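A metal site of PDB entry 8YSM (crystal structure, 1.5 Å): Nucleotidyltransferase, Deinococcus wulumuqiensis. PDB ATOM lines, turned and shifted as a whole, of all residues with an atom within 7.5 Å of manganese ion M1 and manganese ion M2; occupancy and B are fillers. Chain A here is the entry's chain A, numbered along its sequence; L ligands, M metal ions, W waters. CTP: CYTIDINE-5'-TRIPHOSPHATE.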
ATOM      1  N   GLN A  60     -14.091 -17.430 -26.618  1.00  0.00           N
ATOM      2  CA  GLN A  60     -14.288 -18.890 -26.465  1.00  0.00           C
ATOM      3  C   GLN A  60     -15.452 -19.323 -27.320  1.00  0.00           C
ATOM      4  O   GLN A  60     -16.181 -18.458 -27.830  1.00  0.00           O
ATOM      5  CB  GLN A  60     -14.648 -19.300 -25.036  1.00  0.00           C
ATOM      6  CG  GLN A  60     -13.524 -19.172 -24.067  1.00  0.00           C
ATOM      7  CD  GLN A  60     -13.891 -19.773 -22.743  1.00  0.00           C
ATOM      8  OE1 GLN A  60     -15.057 -20.001 -22.432  1.00  0.00           O
ATOM      9  NE2 GLN A  60     -12.927 -19.889 -21.881  1.00  0.00           N
ATOM     10  N   GLY A  61     -15.595 -20.606 -27.486  1.00  0.00           N
ATOM     11  CA  GLY A  61     -16.816 -21.147 -28.054  1.00  0.00           C
ATOM     12  C   GLY A  61     -16.900 -21.006 -29.565  1.00  0.00           C
ATOM     13  O   GLY A  61     -15.910 -20.627 -30.241  1.00  0.00           O
ATOM     14  N   SER A  62     -18.072 -21.211 -30.089  1.00  0.00           N
ATOM     15  CA  SER A  62     -18.284 -21.320 -31.555  1.00  0.00           C
ATOM     16  C   SER A  62     -17.988 -19.981 -32.231  1.00  0.00           C
ATOM     17  O   SER A  62     -17.507 -19.983 -33.361  1.00  0.00           O
ATOM     18  CB  SER A  62     -19.652 -21.791 -31.861  1.00  0.00           C
ATOM     19  OG  SER A  62     -20.636 -20.907 -31.408  1.00  0.00           O
ATOM     20  N   TYR A  63     -18.199 -18.850 -31.559  1.00  0.00           N
ATOM     21  CA  TYR A  63     -17.951 -17.545 -32.188  1.00  0.00           C
ATOM     22  C   TYR A  63     -16.461 -17.290 -32.287  1.00  0.00           C
ATOM     23  O   TYR A  63     -16.081 -16.501 -33.127  1.00  0.00           O
ATOM     24  CB  TYR A  63     -18.731 -16.473 -31.409  1.00  0.00           C
ATOM     25  CG  TYR A  63     -20.225 -16.696 -31.272  1.00  0.00           C
ATOM     26  CD1 TYR A  63     -20.983 -15.858 -30.469  1.00  0.00           C
ATOM     27  CD2 TYR A  63     -20.914 -17.732 -31.915  1.00  0.00           C
ATOM     28  CE1 TYR A  63     -22.340 -16.006 -30.311  1.00  0.00           C
ATOM     29  CE2 TYR A  63     -22.294 -17.860 -31.802  1.00  0.00           C
ATOM     30  CZ  TYR A  63     -23.004 -17.020 -30.955  1.00  0.00           C
ATOM     31  OH  TYR A  63     -24.370 -17.135 -30.787  1.00  0.00           O
ATOM     32  N   MET A  65     -14.378 -19.975 -32.911  1.00  0.00           N
ATOM     33  CA  MET A  65     -13.926 -21.080 -33.781  1.00  0.00           C
ATOM     34  C   MET A  65     -14.565 -21.004 -35.180  1.00  0.00           C
ATOM     35  O   MET A  65     -14.251 -21.899 -36.044  1.00  0.00           O
ATOM     36  CB  MET A  65     -14.250 -22.433 -33.123  1.00  0.00           C
ATOM     37  CG  MET A  65     -13.550 -22.638 -31.806  1.00  0.00           C
ATOM     38  SD  MET A  65     -13.724 -24.262 -31.116  1.00  0.00           S
ATOM     39  CE  MET A  65     -15.427 -24.214 -30.630  1.00  0.00           C
ATOM     40  N   TYR A  77     -28.687 -16.057 -29.044  1.00  0.00           N
ATOM     41  CA  TYR A  77     -27.221 -16.065 -29.307  1.00  0.00           C
ATOM     42  C   TYR A  77     -26.519 -16.527 -28.014  1.00  0.00           C
ATOM     43  O   TYR A  77     -27.011 -16.301 -26.926  1.00  0.00           O
ATOM     44  CB  TYR A  77     -26.777 -14.695 -29.809  1.00  0.00           C
ATOM     45  CG  TYR A  77     -27.251 -14.370 -31.208  1.00  0.00           C
ATOM     46  CD1 TYR A  77     -28.494 -13.824 -31.471  1.00  0.00           C
ATOM     47  CD2 TYR A  77     -26.474 -14.728 -32.283  1.00  0.00           C
ATOM     48  CE1 TYR A  77     -28.918 -13.590 -32.776  1.00  0.00           C
ATOM     49  CE2 TYR A  77     -26.858 -14.484 -33.579  1.00  0.00           C
ATOM     50  CZ  TYR A  77     -28.094 -13.928 -33.849  1.00  0.00           C
ATOM     51  OH  TYR A  77     -28.448 -13.755 -35.161  1.00  0.00           O
ATOM     52  N   ASP A  78     -25.404 -17.236 -28.166  1.00  0.00           N
ATOM     53  CA  ASP A  78     -24.632 -17.827 -27.057  1.00  0.00           C
ATOM     54  C   ASP A  78     -23.243 -17.222 -27.104  1.00  0.00           C
ATOM     55  O   ASP A  78     -22.405 -17.761 -27.791  1.00  0.00           O
ATOM     56  CB  ASP A  78     -24.557 -19.355 -27.178  1.00  0.00           C
ATOM     57  CG  ASP A  78     -23.737 -19.963 -26.062  1.00  0.00           C
ATOM     58  OD1 ASP A  78     -23.854 -19.468 -24.938  1.00  0.00           O
ATOM     59  OD2 ASP A  78     -23.031 -20.958 -26.317  1.00  0.00           O
ATOM     60  N   ILE A  79     -22.998 -16.092 -26.412  1.00  0.00           N
ATOM     61  CA  ILE A  79     -21.711 -15.373 -26.486  1.00  0.00           C
ATOM     62  C   ILE A  79     -20.788 -15.948 -25.398  1.00  0.00           C
ATOM     63  O   ILE A  79     -21.038 -15.690 -24.227  1.00  0.00           O
ATOM     64  CB  ILE A  79     -21.946 -13.858 -26.336  1.00  0.00           C
ATOM     65  CG1 ILE A  79     -22.776 -13.302 -27.489  1.00  0.00           C
ATOM     66  CG2 ILE A  79     -20.614 -13.128 -26.194  1.00  0.00           C
ATOM     67  CD1 ILE A  79     -23.077 -11.800 -27.388  1.00  0.00           C
ATOM     68  N   ASP A  80     -19.810 -16.783 -25.774  1.00  0.00           N
ATOM     69  CA  ASP A  80     -18.890 -17.440 -24.827  1.00  0.00           C
ATOM     70  C   ASP A  80     -17.615 -16.635 -24.701  1.00  0.00           C
ATOM     71  O   ASP A  80     -17.021 -16.269 -25.714  1.00  0.00           O
ATOM     72  CB  ASP A  80     -18.587 -18.863 -25.224  1.00  0.00           C
ATOM     73  CG  ASP A  80     -19.819 -19.749 -25.370  1.00  0.00           C
ATOM     74  OD1 ASP A  80     -19.961 -20.382 -26.466  1.00  0.00           O
ATOM     75  OD2 ASP A  80     -20.676 -19.745 -24.458  1.00  0.00           O
ATOM     76  N   VAL A  81     -17.209 -16.319 -23.456  1.00  0.00           N
ATOM     77  CA  VAL A  81     -15.976 -15.533 -23.203  1.00  0.00           C
ATOM     78  C   VAL A  81     -15.325 -16.074 -21.930  1.00  0.00           C
ATOM     79  O   VAL A  81     -16.021 -16.628 -21.100  1.00  0.00           O
ATOM     80  CB  VAL A  81     -16.294 -14.019 -23.127  1.00  0.00           C
ATOM     81  CG1 VAL A  81     -17.132 -13.685 -21.924  1.00  0.00           C
ATOM     82  CG2 VAL A  81     -15.047 -13.159 -23.179  1.00  0.00           C
ATOM     83  N   ARG A 115     -23.670 -20.880 -12.886  1.00  0.00           N
ATOM     84  CA  ARG A 115     -23.850 -22.236 -13.438  1.00  0.00           C
ATOM     85  C   ARG A 115     -22.629 -23.069 -13.048  1.00  0.00           C
ATOM     86  O   ARG A 115     -21.670 -22.507 -12.504  1.00  0.00           O
ATOM     87  CB  ARG A 115     -24.077 -22.144 -14.953  1.00  0.00           C
ATOM     88  CG  ARG A 115     -25.169 -21.159 -15.373  1.00  0.00           C
ATOM     89  CD  ARG A 115     -26.343 -21.873 -15.988  1.00  0.00           C
ATOM     90  NE  ARG A 115     -27.347 -21.017 -16.616  1.00  0.00           N
ATOM     91  CZ  ARG A 115     -27.431 -20.764 -17.933  1.00  0.00           C
ATOM     92  NH1 ARG A 115     -26.493 -21.206 -18.765  1.00  0.00           N
ATOM     93  NH2 ARG A 115     -28.436 -20.045 -18.398  1.00  0.00           N
ATOM     94  N   CYS A 118     -19.802 -21.694 -15.470  1.00  0.00           N
ATOM     95  CA  CYS A 118     -19.741 -20.287 -15.908  1.00  0.00           C
ATOM     96  C   CYS A 118     -20.674 -19.445 -15.065  1.00  0.00           C
ATOM     97  O   CYS A 118     -21.526 -20.012 -14.335  1.00  0.00           O
ATOM     98  CB  CYS A 118     -20.075 -20.141 -17.389  1.00  0.00           C
ATOM     99  SG  CYS A 118     -21.752 -20.689 -17.827  1.00  0.00           S
ATOM    100  N   THR A 120     -23.626 -16.851 -16.146  1.00  0.00           N
ATOM    101  CA  THR A 120     -24.407 -16.511 -17.349  1.00  0.00           C
ATOM    102  C   THR A 120     -25.182 -15.243 -17.066  1.00  0.00           C
ATOM    103  O   THR A 120     -25.864 -15.208 -16.027  1.00  0.00           O
ATOM    104  CB  THR A 120     -25.337 -17.659 -17.750  1.00  0.00           C
ATOM    105  OG1 THR A 120     -24.526 -18.805 -18.037  1.00  0.00           O
ATOM    106  CG2 THR A 120     -26.215 -17.293 -18.908  1.00  0.00           C
ATOM    107  N   HIS A 127     -27.572 -14.535 -24.456  1.00  0.00           N
ATOM    108  CA  HIS A 127     -26.900 -14.651 -23.151  1.00  0.00           C
ATOM    109  C   HIS A 127     -25.392 -14.669 -23.349  1.00  0.00           C
ATOM    110  O   HIS A 127     -24.897 -14.992 -24.488  1.00  0.00           O
ATOM    111  CB  HIS A 127     -27.402 -15.867 -22.393  1.00  0.00           C
ATOM    112  CG  HIS A 127     -27.248 -17.149 -23.131  1.00  0.00           C
ATOM    113  ND1 HIS A 127     -28.230 -17.650 -23.961  1.00  0.00           N
ATOM    114  CD2 HIS A 127     -26.238 -18.044 -23.144  1.00  0.00           C
ATOM    115  CE1 HIS A 127     -27.810 -18.781 -24.477  1.00  0.00           C
ATOM    116  NE2 HIS A 127     -26.603 -19.045 -23.982  1.00  0.00           N
ATOM    117  N   VAL A 128     -24.680 -14.270 -22.316  1.00  0.00           N
ATOM    118  CA  VAL A 128     -23.204 -14.257 -22.271  1.00  0.00           C
ATOM    119  C   VAL A 128     -22.771 -15.221 -21.174  1.00  0.00           C
ATOM    120  O   VAL A 128     -23.229 -15.087 -20.031  1.00  0.00           O
ATOM    121  CB  VAL A 128     -22.650 -12.845 -22.042  1.00  0.00           C
ATOM    122  CG1 VAL A 128     -21.134 -12.859 -21.919  1.00  0.00           C
ATOM    123  CG2 VAL A 128     -23.114 -11.865 -23.105  1.00  0.00           C
ATOM    124  N   ASP A 129     -21.994 -16.226 -21.554  1.00  0.00           N
ATOM    125  CA  ASP A 129     -21.469 -17.260 -20.646  1.00  0.00           C
ATOM    126  C   ASP A 129     -20.033 -16.879 -20.349  1.00  0.00           C
ATOM    127  O   ASP A 129     -19.170 -17.013 -21.285  1.00  0.00           O
ATOM    128  CB  ASP A 129     -21.556 -18.664 -21.251  1.00  0.00           C
ATOM    129  CG  ASP A 129     -22.962 -19.168 -21.431  1.00  0.00           C
ATOM    130  OD1 ASP A 129     -23.888 -18.536 -20.883  1.00  0.00           O
ATOM    131  OD2 ASP A 129     -23.123 -20.167 -22.141  1.00  0.00           O
ATOM    132  N   LEU A 130     -19.756 -16.427 -19.128  1.00  0.00           N
ATOM    133  CA  LEU A 130     -18.379 -16.132 -18.677  1.00  0.00           C
ATOM    134  C   LEU A 130     -17.816 -17.323 -17.936  1.00  0.00           C
ATOM    135  O   LEU A 130     -18.222 -17.596 -16.793  1.00  0.00           O
ATOM    136  CB  LEU A 130     -18.351 -14.896 -17.775  1.00  0.00           C
ATOM    137  CG  LEU A 130     -19.012 -13.663 -18.356  1.00  0.00           C
ATOM    138  CD1 LEU A 130     -20.446 -13.566 -17.877  1.00  0.00           C
ATOM    139  CD2 LEU A 130     -18.223 -12.443 -17.981  1.00  0.00           C
ATOM    140  N   LYS A 191     -25.684 -28.440 -35.949  1.00  0.00           N
ATOM    141  CA  LYS A 191     -26.211 -27.506 -34.923  1.00  0.00           C
ATOM    142  C   LYS A 191     -27.609 -27.033 -35.340  1.00  0.00           C
ATOM    143  O   LYS A 191     -28.471 -26.886 -34.454  1.00  0.00           O
ATOM    144  CB  LYS A 191     -25.289 -26.321 -34.748  1.00  0.00           C
ATOM    145  CG  LYS A 191     -24.031 -26.656 -34.007  1.00  0.00           C
ATOM    146  CD  LYS A 191     -23.154 -25.456 -33.825  1.00  0.00           C
ATOM    147  CE  LYS A 191     -21.939 -25.764 -33.034  1.00  0.00           C
ATOM    148  NZ  LYS A 191     -21.141 -24.542 -32.917  1.00  0.00           N
ATOM    149  N   ARG A 194     -29.870 -29.915 -34.625  1.00  0.00           N
ATOM    150  CA  ARG A 194     -30.065 -29.925 -33.166  1.00  0.00           C
ATOM    151  C   ARG A 194     -31.138 -28.918 -32.785  1.00  0.00           C
ATOM    152  O   ARG A 194     -32.085 -29.275 -32.056  1.00  0.00           O
ATOM    153  CB  ARG A 194     -28.765 -29.614 -32.452  1.00  0.00           C
ATOM    154  CG  ARG A 194     -28.922 -29.357 -30.959  1.00  0.00           C
ATOM    155  CD  ARG A 194     -27.813 -28.583 -30.387  1.00  0.00           C
ATOM    156  NE  ARG A 194     -27.716 -27.241 -30.949  1.00  0.00           N
ATOM    157  CZ  ARG A 194     -26.641 -26.460 -30.802  1.00  0.00           C
ATOM    158  NH1 ARG A 194     -25.609 -26.889 -30.078  1.00  0.00           N
ATOM    159  NH2 ARG A 194     -26.632 -25.271 -31.354  1.00  0.00           N
ATOM    160  N   GLY A 208     -23.309 -28.092 -28.358  1.00  0.00           N
ATOM    161  CA  GLY A 208     -22.454 -27.690 -29.472  1.00  0.00           C
ATOM    162  C   GLY A 208     -21.044 -28.205 -29.317  1.00  0.00           C
ATOM    163  O   GLY A 208     -20.460 -28.622 -30.303  1.00  0.00           O
ATOM    164  N   ILE A 209     -20.457 -28.126 -28.129  1.00  0.00           N
ATOM    165  CA  ILE A 209     -19.080 -28.613 -27.910  1.00  0.00           C
ATOM    166  C   ILE A 209     -19.016 -30.109 -28.213  1.00  0.00           C
ATOM    167  O   ILE A 209     -17.978 -30.592 -28.675  1.00  0.00           O
ATOM    168  CB  ILE A 209     -18.522 -28.247 -26.506  1.00  0.00           C
ATOM    169  CG1 ILE A 209     -17.018 -28.524 -26.441  1.00  0.00           C
ATOM    170  CG2 ILE A 209     -19.293 -28.952 -25.381  1.00  0.00           C
ATOM    171  CD1 ILE A 209     -16.341 -27.958 -25.198  1.00  0.00           C
HETATM  172  N1  CTP L   1     -14.694 -25.486 -23.131  1.00  0.00           N
HETATM  173  C2  CTP L   1     -13.793 -25.241 -24.176  1.00  0.00           C
HETATM  174  N3  CTP L   1     -12.666 -25.991 -24.253  1.00  0.00           N
HETATM  175  C4  CTP L   1     -12.373 -26.869 -23.295  1.00  0.00           C
HETATM  176  C5  CTP L   1     -13.259 -27.108 -22.201  1.00  0.00           C
HETATM  177  C6  CTP L   1     -14.396 -26.408 -22.162  1.00  0.00           C
HETATM  178  O2  CTP L   1     -14.077 -24.404 -25.074  1.00  0.00           O
HETATM  179  N4  CTP L   1     -11.244 -27.541 -23.410  1.00  0.00           N
HETATM  180  C1' CTP L   1     -15.909 -24.622 -22.976  1.00  0.00           C
HETATM  181  C2' CTP L   1     -15.570 -23.108 -23.038  1.00  0.00           C
HETATM  182  O2' CTP L   1     -15.796 -22.567 -21.745  1.00  0.00           O
HETATM  183  C3' CTP L   1     -16.509 -22.594 -24.157  1.00  0.00           C
HETATM  184  C4' CTP L   1     -17.596 -23.654 -24.156  1.00  0.00           C
HETATM  185  O4' CTP L   1     -16.842 -24.874 -23.989  1.00  0.00           O
HETATM  186  O3' CTP L   1     -17.097 -21.315 -23.950  1.00  0.00           O
HETATM  187  C5' CTP L   1     -18.440 -23.730 -25.378  1.00  0.00           C
HETATM  188  O5' CTP L   1     -19.363 -24.817 -25.231  1.00  0.00           O
HETATM  189  PA  CTP L   1     -20.657 -24.724 -26.168  1.00  0.00           P
HETATM  190  O1A CTP L   1     -21.527 -25.957 -25.960  1.00  0.00           O
HETATM  191  O2A CTP L   1     -21.251 -23.355 -26.048  1.00  0.00           O
HETATM  192  O3A CTP L   1     -19.987 -24.973 -27.578  1.00  0.00           O
HETATM  193  PB  CTP L   1     -19.964 -24.086 -28.854  1.00  0.00           P
HETATM  194  O1B CTP L   1     -18.829 -24.644 -29.657  1.00  0.00           O
HETATM  195  O2B CTP L   1     -19.939 -22.578 -28.485  1.00  0.00           O
HETATM  196  O3B CTP L   1     -21.369 -24.520 -29.532  1.00  0.00           O
HETATM  197  PG  CTP L   1     -22.732 -23.677 -29.858  1.00  0.00           P
HETATM  198  O1G CTP L   1     -22.884 -22.757 -28.643  1.00  0.00           O
HETATM  199  O2G CTP L   1     -23.759 -24.736 -29.966  1.00  0.00           O
HETATM  200  O3G CTP L   1     -22.417 -22.980 -31.110  1.00  0.00           O
HETATM  201 MN    MN M   1     -22.401 -20.878 -23.933  1.00  0.00          MN
HETATM  202 MN    MN M   2     -21.478 -21.583 -27.479  1.00  0.00          MN
HETATM  203  O   HOH W   1     -20.829 -22.107 -23.047  1.00  0.00           O
HETATM  204  O   HOH W   2     -21.404 -19.869 -28.929  1.00  0.00           O
HETATM  205  O   HOH W   3     -24.053 -22.327 -23.855  1.00  0.00           O
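Two residues have an atom within 4 Å of manganese ion M2: Asp 78 and Asp 80. The nearest printed residue that does not touch manganese ion M2 is Ser 62 (4.1 Å).
Manganese ion M2 is bound by the side-chain carboxylate of Asp 78 (2.0 Å), an oxygen (O2B) of the ligand (2.1 Å), an oxygen (O1G) of the ligand (2.2 Å), the side-chain carboxylate of Asp 80 (2.2 Å), water W2 (2.2 Å) and an oxygen (O2A) of the ligand (2.3 Å).
Water W2 lies within hydrogen-bond range of O of Asp 78 and OG of Ser 62.
The backbone NH (N) of Ser 62 sits close to an oxygen (O2B) of the ligand (2.8 Å). An oxygen (O3G) of the ligand is in hydrogen-bond range of the side-chain hydroxyl (OG) of Ser 62 (2.7 Å). The side-chain amide oxygen (OE1) of Gln 60 is in hydrogen-bond range of an oxygen (O2') of the ligand (2.8 Å). NZ of Lys 191 is in salt-bridge range of O3G of the ligand, at 2.7 Å. The backbone NH of Ile 209 sits at hydrogen-bond distance from an oxygen (O3A) of the ligand (3.2 Å). An oxygen (O2G) of the ligand lies within salt-bridge range of the guanidinium group (NH1) of Arg 194.
OD1 of Asp 78 lies close to NE2 of His 127, at 2.9 Å. OH of Tyr 63 is in hydrogen-bond range of N of Asp 78 (2.8 Å). The backbone NH (N) of Asp 129 sits at hydrogen-bond distance from the backbone carbonyl oxygen (O) of Ile 79 (2.9 Å). OG1 of Thr 120 sits at hydrogen-bond distance from OD1 of Asp 129, 2.9 Å away. The backbone carbonyl oxygen of Asp 129 sits at hydrogen-bond distance from the backbone NH of Val 81 (3.0 Å). The backbone carbonyl oxygen of Asp 80 sits at hydrogen-bond distance from the backbone NH of Gln 60 (3.3 Å).
Three residues have an atom within 4 Å of manganese ion M1: Asp 78, Asp 80 and Asp 129.
Manganese ion M1 is bound by OD2 of Asp 129, 2.1 Å away. OD2 of Asp 80 is bound to manganese ion M1 (2.1 Å). Manganese ion M1 is bound by water W1, 2.2 Å away. Manganese ion M1 is bound by water W3. OD1 of Asp 78 is bound to manganese ion M1. The side-chain carboxylate (OD2) of Asp 78 binds manganese ion M1, at 2.5 Å.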
